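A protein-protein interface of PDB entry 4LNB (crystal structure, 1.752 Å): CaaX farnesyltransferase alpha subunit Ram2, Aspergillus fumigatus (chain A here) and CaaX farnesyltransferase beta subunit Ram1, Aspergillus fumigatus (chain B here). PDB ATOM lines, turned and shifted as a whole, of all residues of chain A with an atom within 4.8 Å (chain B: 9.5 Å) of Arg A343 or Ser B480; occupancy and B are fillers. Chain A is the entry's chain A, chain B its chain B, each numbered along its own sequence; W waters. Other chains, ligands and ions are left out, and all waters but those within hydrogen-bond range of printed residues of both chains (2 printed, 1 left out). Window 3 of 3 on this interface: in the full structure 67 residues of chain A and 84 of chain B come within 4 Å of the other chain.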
ATOM      1  N   LYS A 335       4.319  -3.644 -10.939  1.00  0.00           N
ATOM      2  CA  LYS A 335       5.564  -3.394 -10.223  1.00  0.00           C
ATOM      3  C   LYS A 335       5.751  -4.303  -9.012  1.00  0.00           C
ATOM      4  O   LYS A 335       6.880  -4.577  -8.607  1.00  0.00           O
ATOM      5  CB  LYS A 335       5.690  -1.919  -9.829  1.00  0.00           C
ATOM      6  CG  LYS A 335       4.863  -1.512  -8.638  1.00  0.00           C
ATOM      7  CD  LYS A 335       5.127  -0.063  -8.274  1.00  0.00           C
ATOM      8  CE  LYS A 335       4.612   0.247  -6.884  1.00  0.00           C
ATOM      9  NZ  LYS A 335       4.853   1.665  -6.511  1.00  0.00           N
ATOM     10  N   GLU A 336       4.651  -4.786  -8.441  1.00  0.00           N
ATOM     11  CA  GLU A 336       4.738  -5.597  -7.232  1.00  0.00           C
ATOM     12  C   GLU A 336       4.646  -7.103  -7.476  1.00  0.00           C
ATOM     13  O   GLU A 336       5.161  -7.891  -6.685  1.00  0.00           O
ATOM     14  CB  GLU A 336       3.683  -5.158  -6.209  1.00  0.00           C
ATOM     15  CG  GLU A 336       3.916  -3.761  -5.656  1.00  0.00           C
ATOM     16  CD  GLU A 336       2.879  -3.354  -4.630  1.00  0.00           C
ATOM     17  OE1 GLU A 336       1.923  -4.129  -4.408  1.00  0.00           O
ATOM     18  OE2 GLU A 336       3.020  -2.260  -4.045  1.00  0.00           O
ATOM     19  N   ASP A 339       5.360  -7.949 -13.267  1.00  0.00           N
ATOM     20  CA  ASP A 339       6.594  -7.639 -13.998  1.00  0.00           C
ATOM     21  C   ASP A 339       7.501  -6.734 -13.155  1.00  0.00           C
ATOM     22  O   ASP A 339       7.807  -5.608 -13.555  1.00  0.00           O
ATOM     23  CB  ASP A 339       6.273  -6.965 -15.337  1.00  0.00           C
ATOM     24  CG  ASP A 339       7.362  -7.175 -16.379  1.00  0.00           C
ATOM     25  OD1 ASP A 339       8.492  -7.549 -15.999  1.00  0.00           O
ATOM     26  OD2 ASP A 339       7.086  -6.965 -17.581  1.00  0.00           O
ATOM     27  N   PRO A 340       7.940  -7.227 -11.982  1.00  0.00           N
ATOM     28  CA  PRO A 340       8.599  -6.367 -10.990  1.00  0.00           C
ATOM     29  C   PRO A 340       9.987  -5.859 -11.380  1.00  0.00           C
ATOM     30  O   PRO A 340      10.434  -4.872 -10.802  1.00  0.00           O
ATOM     31  CB  PRO A 340       8.698  -7.268  -9.749  1.00  0.00           C
ATOM     32  CG  PRO A 340       7.729  -8.389  -9.997  1.00  0.00           C
ATOM     33  CD  PRO A 340       7.772  -8.598 -11.475  1.00  0.00           C
ATOM     34  N   ILE A 341      10.664  -6.505 -12.324  1.00  0.00           N
ATOM     35  CA  ILE A 341      11.997  -6.043 -12.706  1.00  0.00           C
ATOM     36  C   ILE A 341      11.932  -4.690 -13.422  1.00  0.00           C
ATOM     37  O   ILE A 341      12.920  -3.957 -13.479  1.00  0.00           O
ATOM     38  CB  ILE A 341      12.758  -7.086 -13.573  1.00  0.00           C
ATOM     39  CG1 ILE A 341      14.271  -6.861 -13.480  1.00  0.00           C
ATOM     40  CG2 ILE A 341      12.291  -7.040 -15.023  1.00  0.00           C
ATOM     41  CD1 ILE A 341      14.831  -7.035 -12.091  1.00  0.00           C
ATOM     42  N   ARG A 342      10.757  -4.350 -13.948  1.00  0.00           N
ATOM     43  CA  ARG A 342      10.582  -3.088 -14.661  1.00  0.00           C
ATOM     44  C   ARG A 342       9.918  -2.039 -13.771  1.00  0.00           C
ATOM     45  O   ARG A 342       9.311  -1.082 -14.259  1.00  0.00           O
ATOM     46  CB  ARG A 342       9.781  -3.310 -15.947  1.00  0.00           C
ATOM     47  CG  ARG A 342      10.450  -4.287 -16.910  1.00  0.00           C
ATOM     48  CD  ARG A 342       9.516  -4.713 -18.036  1.00  0.00           C
ATOM     49  NE  ARG A 342       9.064  -3.582 -18.841  1.00  0.00           N
ATOM     50  CZ  ARG A 342       8.036  -3.631 -19.684  1.00  0.00           C
ATOM     51  NH1 ARG A 342       7.349  -4.754 -19.830  1.00  0.00           N
ATOM     52  NH2 ARG A 342       7.689  -2.554 -20.376  1.00  0.00           N
ATOM     53  N   ARG A 343      10.065  -2.228 -12.463  1.00  0.00           N
ATOM     54  CA  ARG A 343       9.448  -1.369 -11.454  1.00  0.00           C
ATOM     55  C   ARG A 343       9.720   0.117 -11.686  1.00  0.00           C
ATOM     56  O   ARG A 343       8.819   0.942 -11.553  1.00  0.00           O
ATOM     57  CB  ARG A 343       9.931  -1.772 -10.058  1.00  0.00           C
ATOM     58  CG  ARG A 343       9.332  -0.951  -8.927  1.00  0.00           C
ATOM     59  CD  ARG A 343       9.793  -1.467  -7.572  1.00  0.00           C
ATOM     60  NE  ARG A 343       9.125  -0.776  -6.473  1.00  0.00           N
ATOM     61  CZ  ARG A 343       8.131  -1.292  -5.756  1.00  0.00           C
ATOM     62  NH1 ARG A 343       7.689  -2.515  -6.011  1.00  0.00           N
ATOM     63  NH2 ARG A 343       7.583  -0.586  -4.776  1.00  0.00           N
ATOM     64  N   ASN A 344      10.954   0.456 -12.045  1.00  0.00           N
ATOM     65  CA  ASN A 344      11.313   1.859 -12.228  1.00  0.00           C
ATOM     66  C   ASN A 344      10.622   2.513 -13.420  1.00  0.00           C
ATOM     67  O   ASN A 344      10.311   3.708 -13.382  1.00  0.00           O
ATOM     68  CB  ASN A 344      12.832   2.037 -12.293  1.00  0.00           C
ATOM     69  CG  ASN A 344      13.492   1.834 -10.944  1.00  0.00           C
ATOM     70  OD1 ASN A 344      12.909   2.151  -9.907  1.00  0.00           O
ATOM     71  ND2 ASN A 344      14.704   1.299 -10.949  1.00  0.00           N
ATOM     72  N   TYR A 345      10.375   1.729 -14.467  1.00  0.00           N
ATOM     73  CA  TYR A 345       9.572   2.205 -15.589  1.00  0.00           C
ATOM     74  C   TYR A 345       8.099   2.345 -15.201  1.00  0.00           C
ATOM     75  O   TYR A 345       7.458   3.341 -15.533  1.00  0.00           O
ATOM     76  CB  TYR A 345       9.718   1.304 -16.820  1.00  0.00           C
ATOM     77  CG  TYR A 345       8.765   1.692 -17.930  1.00  0.00           C
ATOM     78  CD1 TYR A 345       8.929   2.884 -18.630  1.00  0.00           C
ATOM     79  CD2 TYR A 345       7.690   0.880 -18.264  1.00  0.00           C
ATOM     80  CE1 TYR A 345       8.049   3.250 -19.638  1.00  0.00           C
ATOM     81  CE2 TYR A 345       6.807   1.240 -19.269  1.00  0.00           C
ATOM     82  CZ  TYR A 345       6.991   2.424 -19.950  1.00  0.00           C
ATOM     83  OH  TYR A 345       6.111   2.779 -20.947  1.00  0.00           O
ATOM     84  N   TRP A 346       7.560   1.354 -14.496  1.00  0.00           N
ATOM     85  CA  TRP A 346       6.176   1.443 -14.032  1.00  0.00           C
ATOM     86  C   TRP A 346       5.966   2.670 -13.136  1.00  0.00           C
ATOM     87  O   TRP A 346       4.956   3.364 -13.251  1.00  0.00           O
ATOM     88  CB  TRP A 346       5.741   0.171 -13.295  1.00  0.00           C
ATOM     89  CG  TRP A 346       5.941  -1.126 -14.063  1.00  0.00           C
ATOM     90  CD1 TRP A 346       6.515  -2.268 -13.587  1.00  0.00           C
ATOM     91  CD2 TRP A 346       5.566  -1.405 -15.425  1.00  0.00           C
ATOM     92  NE1 TRP A 346       6.523  -3.239 -14.561  1.00  0.00           N
ATOM     93  CE2 TRP A 346       5.947  -2.737 -15.697  1.00  0.00           C
ATOM     94  CE3 TRP A 346       4.945  -0.662 -16.435  1.00  0.00           C
ATOM     95  CZ2 TRP A 346       5.731  -3.339 -16.938  1.00  0.00           C
ATOM     96  CZ3 TRP A 346       4.731  -1.264 -17.672  1.00  0.00           C
ATOM     97  CH2 TRP A 346       5.125  -2.587 -17.909  1.00  0.00           C
ATOM     98  N   GLU A 347       6.925   2.935 -12.254  1.00  0.00           N
ATOM     99  CA  GLU A 347       6.856   4.094 -11.363  1.00  0.00           C
ATOM    100  C   GLU A 347       6.921   5.403 -12.141  1.00  0.00           C
ATOM    101  O   GLU A 347       6.236   6.367 -11.804  1.00  0.00           O
ATOM    102  CB  GLU A 347       7.979   4.056 -10.324  1.00  0.00           C
ATOM    103  CG  GLU A 347       7.867   2.934  -9.308  1.00  0.00           C
ATOM    104  CD  GLU A 347       6.927   3.262  -8.161  1.00  0.00           C
ATOM    105  OE1 GLU A 347       6.188   4.269  -8.249  1.00  0.00           O
ATOM    106  OE2 GLU A 347       6.934   2.509  -7.164  1.00  0.00           O
ATOM    107  N   LEU B  75      12.481 -12.268  -6.113  1.00  0.00           N
ATOM    108  CA  LEU B  75      12.419 -11.929  -7.536  1.00  0.00           C
ATOM    109  C   LEU B  75      13.527 -12.606  -8.340  1.00  0.00           C
ATOM    110  O   LEU B  75      13.354 -12.913  -9.523  1.00  0.00           O
ATOM    111  CB  LEU B  75      12.500 -10.409  -7.722  1.00  0.00           C
ATOM    112  CG  LEU B  75      12.442  -9.878  -9.157  1.00  0.00           C
ATOM    113  CD1 LEU B  75      11.096 -10.205  -9.791  1.00  0.00           C
ATOM    114  CD2 LEU B  75      12.719  -8.380  -9.199  1.00  0.00           C
ATOM    115  N   PHE B  76      14.661 -12.849  -7.692  1.00  0.00           N
ATOM    116  CA  PHE B  76      15.816 -13.423  -8.375  1.00  0.00           C
ATOM    117  C   PHE B  76      16.040 -14.896  -8.036  1.00  0.00           C
ATOM    118  O   PHE B  76      17.051 -15.479  -8.425  1.00  0.00           O
ATOM    119  CB  PHE B  76      17.067 -12.596  -8.067  1.00  0.00           C
ATOM    120  CG  PHE B  76      16.943 -11.157  -8.477  1.00  0.00           C
ATOM    121  CD1 PHE B  76      16.995 -10.803  -9.817  1.00  0.00           C
ATOM    122  CD2 PHE B  76      16.746 -10.165  -7.530  1.00  0.00           C
ATOM    123  CE1 PHE B  76      16.867  -9.480 -10.202  1.00  0.00           C
ATOM    124  CE2 PHE B  76      16.619  -8.840  -7.910  1.00  0.00           C
ATOM    125  CZ  PHE B  76      16.680  -8.499  -9.244  1.00  0.00           C
ATOM    126  N   TYR B 119      24.407  -8.470  -0.292  1.00  0.00           N
ATOM    127  CA  TYR B 119      23.301  -8.740  -1.207  1.00  0.00           C
ATOM    128  C   TYR B 119      23.380 -10.153  -1.778  1.00  0.00           C
ATOM    129  O   TYR B 119      22.569 -10.535  -2.621  1.00  0.00           O
ATOM    130  CB  TYR B 119      23.269  -7.714  -2.340  1.00  0.00           C
ATOM    131  CG  TYR B 119      22.850  -6.330  -1.900  1.00  0.00           C
ATOM    132  CD1 TYR B 119      21.516  -6.039  -1.641  1.00  0.00           C
ATOM    133  CD2 TYR B 119      23.784  -5.313  -1.757  1.00  0.00           C
ATOM    134  CE1 TYR B 119      21.125  -4.772  -1.244  1.00  0.00           C
ATOM    135  CE2 TYR B 119      23.403  -4.044  -1.361  1.00  0.00           C
ATOM    136  CZ  TYR B 119      22.072  -3.779  -1.105  1.00  0.00           C
ATOM    137  OH  TYR B 119      21.687  -2.518  -0.710  1.00  0.00           O
ATOM    138  N   SER B 346      12.573  -0.919 -21.845  1.00  0.00           N
ATOM    139  CA  SER B 346      12.283  -1.445 -20.518  1.00  0.00           C
ATOM    140  C   SER B 346      12.045  -2.956 -20.559  1.00  0.00           C
ATOM    141  O   SER B 346      12.526  -3.699 -19.697  1.00  0.00           O
ATOM    142  CB  SER B 346      11.059  -0.723 -19.941  1.00  0.00           C
ATOM    143  OG  SER B 346      10.688  -1.258 -18.688  1.00  0.00           O
ATOM    144  N   ALA B 347      11.323  -3.405 -21.581  1.00  0.00           N
ATOM    145  CA  ALA B 347      10.964  -4.814 -21.724  1.00  0.00           C
ATOM    146  C   ALA B 347      12.149  -5.720 -22.052  1.00  0.00           C
ATOM    147  O   ALA B 347      11.994  -6.939 -22.090  1.00  0.00           O
ATOM    148  CB  ALA B 347       9.872  -4.980 -22.779  1.00  0.00           C
ATOM    149  N   GLN B 349      14.668  -6.237 -20.176  1.00  0.00           N
ATOM    150  CA  GLN B 349      15.166  -6.845 -18.942  1.00  0.00           C
ATOM    151  C   GLN B 349      14.228  -7.924 -18.406  1.00  0.00           C
ATOM    152  O   GLN B 349      13.024  -7.707 -18.307  1.00  0.00           O
ATOM    153  CB  GLN B 349      15.390  -5.770 -17.871  1.00  0.00           C
ATOM    154  CG  GLN B 349      16.302  -6.227 -16.744  1.00  0.00           C
ATOM    155  CD  GLN B 349      16.725  -5.091 -15.836  1.00  0.00           C
ATOM    156  OE1 GLN B 349      16.123  -4.015 -15.843  1.00  0.00           O
ATOM    157  NE2 GLN B 349      17.767  -5.327 -15.047  1.00  0.00           N
ATOM    158  N   ALA B 351      13.355 -11.119 -15.399  1.00  0.00           N
ATOM    159  CA  ALA B 351      13.591 -11.700 -14.083  1.00  0.00           C
ATOM    160  C   ALA B 351      13.170 -13.159 -14.171  1.00  0.00           C
ATOM    161  O   ALA B 351      12.198 -13.475 -14.857  1.00  0.00           O
ATOM    162  CB  ALA B 351      12.788 -10.971 -13.017  1.00  0.00           C
ATOM    163  N   VAL B 397      14.832  11.939 -14.097  1.00  0.00           N
ATOM    164  CA  VAL B 397      13.883  10.834 -14.125  1.00  0.00           C
ATOM    165  C   VAL B 397      14.474   9.618 -13.419  1.00  0.00           C
ATOM    166  O   VAL B 397      13.764   8.665 -13.098  1.00  0.00           O
ATOM    167  CB  VAL B 397      13.480  10.458 -15.565  1.00  0.00           C
ATOM    168  CG1 VAL B 397      12.827  11.644 -16.260  1.00  0.00           C
ATOM    169  CG2 VAL B 397      14.692   9.968 -16.354  1.00  0.00           C
ATOM    170  N   GLY B 398      15.778   9.663 -13.168  1.00  0.00           N
ATOM    171  CA  GLY B 398      16.468   8.560 -12.525  1.00  0.00           C
ATOM    172  C   GLY B 398      16.686   7.406 -13.486  1.00  0.00           C
ATOM    173  O   GLY B 398      16.547   7.562 -14.700  1.00  0.00           O
ATOM    174  N   ASN B 399      17.032   6.243 -12.945  1.00  0.00           N
ATOM    175  CA  ASN B 399      17.213   5.054 -13.767  1.00  0.00           C
ATOM    176  C   ASN B 399      15.883   4.350 -13.972  1.00  0.00           C
ATOM    177  O   ASN B 399      15.164   4.086 -13.012  1.00  0.00           O
ATOM    178  CB  ASN B 399      18.224   4.107 -13.121  1.00  0.00           C
ATOM    179  CG  ASN B 399      19.573   4.759 -12.914  1.00  0.00           C
ATOM    180  OD1 ASN B 399      20.260   5.097 -13.876  1.00  0.00           O
ATOM    181  ND2 ASN B 399      19.956   4.945 -11.655  1.00  0.00           N
ATOM    182  N   LEU B 400      15.554   4.051 -15.224  1.00  0.00           N
ATOM    183  CA  LEU B 400      14.254   3.467 -15.536  1.00  0.00           C
ATOM    184  C   LEU B 400      14.322   1.952 -15.720  1.00  0.00           C
ATOM    185  O   LEU B 400      13.356   1.321 -16.153  1.00  0.00           O
ATOM    186  CB  LEU B 400      13.650   4.145 -16.766  1.00  0.00           C
ATOM    187  CG  LEU B 400      13.423   5.649 -16.586  1.00  0.00           C
ATOM    188  CD1 LEU B 400      12.754   6.249 -17.817  1.00  0.00           C
ATOM    189  CD2 LEU B 400      12.605   5.923 -15.336  1.00  0.00           C
ATOM    190  N   TYR B 401      15.470   1.380 -15.379  1.00  0.00           N
ATOM    191  CA  TYR B 401      15.669  -0.064 -15.399  1.00  0.00           C
ATOM    192  C   TYR B 401      16.159  -0.512 -14.023  1.00  0.00           C
ATOM    193  O   TYR B 401      16.333   0.316 -13.126  1.00  0.00           O
ATOM    194  CB  TYR B 401      16.679  -0.452 -16.484  1.00  0.00           C
ATOM    195  CG  TYR B 401      18.089   0.034 -16.223  1.00  0.00           C
ATOM    196  CD1 TYR B 401      19.072  -0.836 -15.765  1.00  0.00           C
ATOM    197  CD2 TYR B 401      18.439   1.361 -16.432  1.00  0.00           C
ATOM    198  CE1 TYR B 401      20.367  -0.397 -15.524  1.00  0.00           C
ATOM    199  CE2 TYR B 401      19.725   1.811 -16.192  1.00  0.00           C
ATOM    200  CZ  TYR B 401      20.686   0.927 -15.741  1.00  0.00           C
ATOM    201  OH  TYR B 401      21.969   1.370 -15.503  1.00  0.00           O
ATOM    202  N   SER B 402      16.382  -1.812 -13.855  1.00  0.00           N
ATOM    203  CA  SER B 402      16.867  -2.341 -12.584  1.00  0.00           C
ATOM    204  C   SER B 402      18.376  -2.530 -12.587  1.00  0.00           C
ATOM    205  O   SER B 402      18.893  -3.468 -13.201  1.00  0.00           O
ATOM    206  CB  SER B 402      16.178  -3.667 -12.239  1.00  0.00           C
ATOM    207  OG  SER B 402      16.771  -4.271 -11.098  1.00  0.00           O
ATOM    208  N   ARG B 403      19.082  -1.633 -11.901  1.00  0.00           N
ATOM    209  CA  ARG B 403      20.530  -1.758 -11.761  1.00  0.00           C
ATOM    210  C   ARG B 403      20.870  -3.014 -10.965  1.00  0.00           C
ATOM    211  O   ARG B 403      21.858  -3.688 -11.252  1.00  0.00           O
ATOM    212  CB  ARG B 403      21.136  -0.513 -11.096  1.00  0.00           C
ATOM    213  CG  ARG B 403      21.144   0.725 -11.987  1.00  0.00           C
ATOM    214  CD  ARG B 403      21.967   1.864 -11.378  1.00  0.00           C
ATOM    215  NE  ARG B 403      21.421   2.310 -10.102  1.00  0.00           N
ATOM    216  CZ  ARG B 403      22.124   2.438  -8.982  1.00  0.00           C
ATOM    217  NH1 ARG B 403      23.423   2.158  -8.963  1.00  0.00           N
ATOM    218  NH2 ARG B 403      21.526   2.852  -7.876  1.00  0.00           N
ATOM    219  N   GLU B 404      20.040  -3.329  -9.972  1.00  0.00           N
ATOM    220  CA  GLU B 404      20.232  -4.541  -9.178  1.00  0.00           C
ATOM    221  C   GLU B 404      20.202  -5.791 -10.052  1.00  0.00           C
ATOM    222  O   GLU B 404      21.090  -6.636  -9.962  1.00  0.00           O
ATOM    223  CB  GLU B 404      19.173  -4.664  -8.076  1.00  0.00           C
ATOM    224  CG  GLU B 404      19.266  -5.982  -7.309  1.00  0.00           C
ATOM    225  CD  GLU B 404      18.296  -6.071  -6.138  1.00  0.00           C
ATOM    226  OE1 GLU B 404      17.430  -5.181  -5.999  1.00  0.00           O
ATOM    227  OE2 GLU B 404      18.404  -7.038  -5.355  1.00  0.00           O
ATOM    228  N   GLY B 405      19.172  -5.902 -10.886  1.00  0.00           N
ATOM    229  CA  GLY B 405      19.023  -7.047 -11.767  1.00  0.00           C
ATOM    230  C   GLY B 405      20.223  -7.234 -12.675  1.00  0.00           C
ATOM    231  O   GLY B 405      20.763  -8.333 -12.788  1.00  0.00           O
ATOM    232  N   LEU B 406      20.651  -6.155 -13.318  1.00  0.00           N
ATOM    233  CA  LEU B 406      21.772  -6.242 -14.244  1.00  0.00           C
ATOM    234  C   LEU B 406      23.049  -6.647 -13.519  1.00  0.00           C
ATOM    235  O   LEU B 406      23.816  -7.481 -14.008  1.00  0.00           O
ATOM    236  CB  LEU B 406      21.984  -4.913 -14.968  1.00  0.00           C
ATOM    237  CG  LEU B 406      23.061  -4.955 -16.048  1.00  0.00           C
ATOM    238  CD1 LEU B 406      22.680  -5.971 -17.115  1.00  0.00           C
ATOM    239  CD2 LEU B 406      23.263  -3.574 -16.653  1.00  0.00           C
ATOM    240  N   SER B 475      25.015   0.783  -2.472  1.00  0.00           N
ATOM    241  CA  SER B 475      23.875   1.060  -1.610  1.00  0.00           C
ATOM    242  C   SER B 475      23.863   0.202  -0.354  1.00  0.00           C
ATOM    243  O   SER B 475      24.650  -0.735  -0.212  1.00  0.00           O
ATOM    244  CB  SER B 475      22.570   0.834  -2.382  1.00  0.00           C
ATOM    245  OG  SER B 475      22.503   1.650  -3.536  1.00  0.00           O
ATOM    246  N   ASP B 476      22.960   0.542   0.558  1.00  0.00           N
ATOM    247  CA  ASP B 476      22.663  -0.294   1.708  1.00  0.00           C
ATOM    248  C   ASP B 476      21.148  -0.470   1.792  1.00  0.00           C
ATOM    249  O   ASP B 476      20.395   0.444   1.457  1.00  0.00           O
ATOM    250  CB  ASP B 476      23.203   0.347   2.987  1.00  0.00           C
ATOM    251  CG  ASP B 476      23.096  -0.571   4.186  1.00  0.00           C
ATOM    252  OD1 ASP B 476      23.248  -1.798   4.012  1.00  0.00           O
ATOM    253  OD2 ASP B 476      22.859  -0.063   5.303  1.00  0.00           O
ATOM    254  N   GLY B 477      20.702  -1.647   2.217  1.00  0.00           N
ATOM    255  CA  GLY B 477      19.280  -1.911   2.355  1.00  0.00           C
ATOM    256  C   GLY B 477      18.580  -2.181   1.035  1.00  0.00           C
ATOM    257  O   GLY B 477      19.220  -2.297  -0.009  1.00  0.00           O
ATOM    258  N   GLN B 478      17.255  -2.281   1.088  1.00  0.00           N
ATOM    259  CA  GLN B 478      16.453  -2.568  -0.096  1.00  0.00           C
ATOM    260  C   GLN B 478      16.001  -1.283  -0.786  1.00  0.00           C
ATOM    261  O   GLN B 478      16.091  -0.196  -0.215  1.00  0.00           O
ATOM    262  CB  GLN B 478      15.238  -3.421   0.276  1.00  0.00           C
ATOM    263  CG  GLN B 478      15.582  -4.825   0.742  1.00  0.00           C
ATOM    264  CD  GLN B 478      14.363  -5.614   1.170  1.00  0.00           C
ATOM    265  OE1 GLN B 478      13.348  -5.037   1.560  1.00  0.00           O
ATOM    266  NE2 GLN B 478      14.457  -6.938   1.098  1.00  0.00           N
ATOM    267  N   GLY B 479      15.516  -1.412  -2.018  1.00  0.00           N
ATOM    268  CA  GLY B 479      15.083  -0.260  -2.786  1.00  0.00           C
ATOM    269  C   GLY B 479      14.945  -0.599  -4.256  1.00  0.00           C
ATOM    270  O   GLY B 479      15.461  -1.619  -4.711  1.00  0.00           O
ATOM    271  N   SER B 480      14.254   0.254  -5.005  1.00  0.00           N
ATOM    272  CA  SER B 480      13.994  -0.023  -6.418  1.00  0.00           C
ATOM    273  C   SER B 480      15.168   0.356  -7.320  1.00  0.00           C
ATOM    274  O   SER B 480      15.313  -0.184  -8.414  1.00  0.00           O
ATOM    275  CB  SER B 480      12.725   0.691  -6.887  1.00  0.00           C
ATOM    276  OG  SER B 480      12.943   2.084  -7.016  1.00  0.00           O
ATOM    277  N   ASP B 481      16.002   1.285  -6.860  1.00  0.00           N
ATOM    278  CA  ASP B 481      17.148   1.740  -7.649  1.00  0.00           C
ATOM    279  C   ASP B 481      18.409   1.752  -6.786  1.00  0.00           C
ATOM    280  O   ASP B 481      18.818   2.796  -6.280  1.00  0.00           O
ATOM    281  CB  ASP B 481      16.869   3.132  -8.228  1.00  0.00           C
ATOM    282  CG  ASP B 481      18.002   3.650  -9.104  1.00  0.00           C
ATOM    283  OD1 ASP B 481      18.704   2.837  -9.746  1.00  0.00           O
ATOM    284  OD2 ASP B 481      18.184   4.884  -9.157  1.00  0.00           O
ATOM    285  N   ILE B 482      19.020   0.582  -6.622  1.00  0.00           N
ATOM    286  CA  ILE B 482      20.159   0.437  -5.718  1.00  0.00           C
ATOM    287  C   ILE B 482      21.392  -0.146  -6.398  1.00  0.00           C
ATOM    288  O   ILE B 482      21.296  -0.850  -7.409  1.00  0.00           O
ATOM    289  CB  ILE B 482      19.811  -0.459  -4.513  1.00  0.00           C
ATOM    290  CG1 ILE B 482      19.239  -1.793  -4.994  1.00  0.00           C
ATOM    291  CG2 ILE B 482      18.830   0.243  -3.583  1.00  0.00           C
ATOM    292  CD1 ILE B 482      18.914  -2.756  -3.871  1.00  0.00           C
ATOM    293  N   GLY B 483      22.554   0.150  -5.825  1.00  0.00           N
ATOM    294  CA  GLY B 483      23.803  -0.414  -6.297  1.00  0.00           C
ATOM    295  C   GLY B 483      24.203  -1.584  -5.422  1.00  0.00           C
ATOM    296  O   GLY B 483      24.594  -1.395  -4.270  1.00  0.00           O
ATOM    297  N   VAL B 484      24.102  -2.793  -5.968  1.00  0.00           N
ATOM    298  CA  VAL B 484      24.349  -4.007  -5.196  1.00  0.00           C
ATOM    299  C   VAL B 484      25.751  -4.573  -5.429  1.00  0.00           C
ATOM    300  O   VAL B 484      26.114  -5.609  -4.875  1.00  0.00           O
ATOM    301  CB  VAL B 484      23.287  -5.080  -5.489  1.00  0.00           C
ATOM    302  CG1 VAL B 484      21.933  -4.625  -4.975  1.00  0.00           C
ATOM    303  CG2 VAL B 484      23.224  -5.366  -6.982  1.00  0.00           C
HETATM  304  O   HOH W   1      17.771   0.655 -10.773  1.00  0.00           O
HETATM  305  O   HOH W   2      10.307  -8.525 -17.824  1.00  0.00           O
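Water W1 lies within hydrogen-bond range of the side-chain carboxylate of Asp B481 (2.6 Å), the backbone carbonyl oxygen of Tyr B401 (2.8 Å), the backbone NH of Arg B403 (2.9 Å) and the side-chain amide nitrogen of Asn A344 (3.1 Å).
Water W2 bridges the side-chain carboxylate (OD1) of Asp A339 and the backbone carbonyl oxygen (O) of Gln B349.
Of the printed residues of chain B, Arg A343 touches Ser B480.
Asn A344 touches five residues of chain B.
Of the printed residues of chain A, Tyr B401 touches Asn A344 (2.9 Å).
Of the printed residues of chain A, Asn B399 touches Asn A344.
Of the printed residues of chain A, Ser B346 touches Arg A342 and Tyr A345.
Of the printed residues of chain A, Phe B76 touches Ile A341.
Printed residues of chain B within 4 Å of Tyr A345: Ser B346 and Leu B400.
The nearest printed residue of chain A that does not touch Ser B346 is Trp A346 (5.7 Å).
ND2 of Asn A344 sits at hydrogen-bond distance from O of Tyr B401.
The backbone NH (N) of Tyr A345 sits at hydrogen-bond distance from the backbone carbonyl oxygen (O) of Leu B400 (3.4 Å).
ND2 of Asn A344 lies close to O of Asn B399, at 3.5 Å.
OG of Ser B346 is in hydrogen-bond range of NE of Arg A342, at 2.8 Å.
The side-chain hydroxyl (OG) of Ser B480 is in hydrogen-bond range of the side-chain amide oxygen (OD1) of Asn A344 (2.9 Å).
Of the 27 printed residues of chain B, 12 touch a printed residue of chain A.
Of the 11 printed residues of chain A, 6 touch a printed residue of chain B.
Printed residues of chain A that touch a printed residue of chain B: Pro A340, Ile A341, Arg A342, Arg A343, Asn A344 and Tyr A345.
Hydrophobic or aromatic side chains of chain A within 4 Å of the printed part of chain B: Pro A340, Ile A341 and Tyr A345.
Among the printed residues, 16 pairs touch across the chains.
CB of Pro A340 touches CD1 of Leu B75, at 3.8 Å.
CD1 of Ile A341 touches CD2 of Leu B75, 3.8 Å away.
Gln B349 touches Ile A341.
CB of Ile A341 touches CB of Ala B351, at 3.9 Å.
CB of Ser B402 touches O of Ile A341, 3.5 Å away.
Arg A342 touches Ala B347.
Ser B480 touches Arg A343 (CB to CD, 3.7 Å).
Asn A344 touches Leu B400 (CB to C, 3.7 Å).
CB of Asp B481 touches ND2 of Asn A344, 3.9 Å away.
Ser B346 touches Tyr A345.
OD2 of Asp A339 is in salt-bridge range of NH1 of Arg A342.
The side-chain amide nitrogen of Gln B349 is in hydrogen-bond range of the backbone carbonyl oxygen of Ser B402 (2.9 Å).
The side-chain hydroxyl of Ser B402 sits at hydrogen-bond distance from the backbone NH of Gly B405 (2.9 Å).
ND2 of Asn B399 sits close to NE of Arg B403, 3.4 Å away.
The side-chain amide nitrogen of Asn B399 lies within hydrogen-bond range of the side-chain carboxylate of Asp B481 (3.1 Å).
The side-chain amide nitrogen of Gln B349 lies close to the backbone NH of Leu B406 (3.5 Å).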
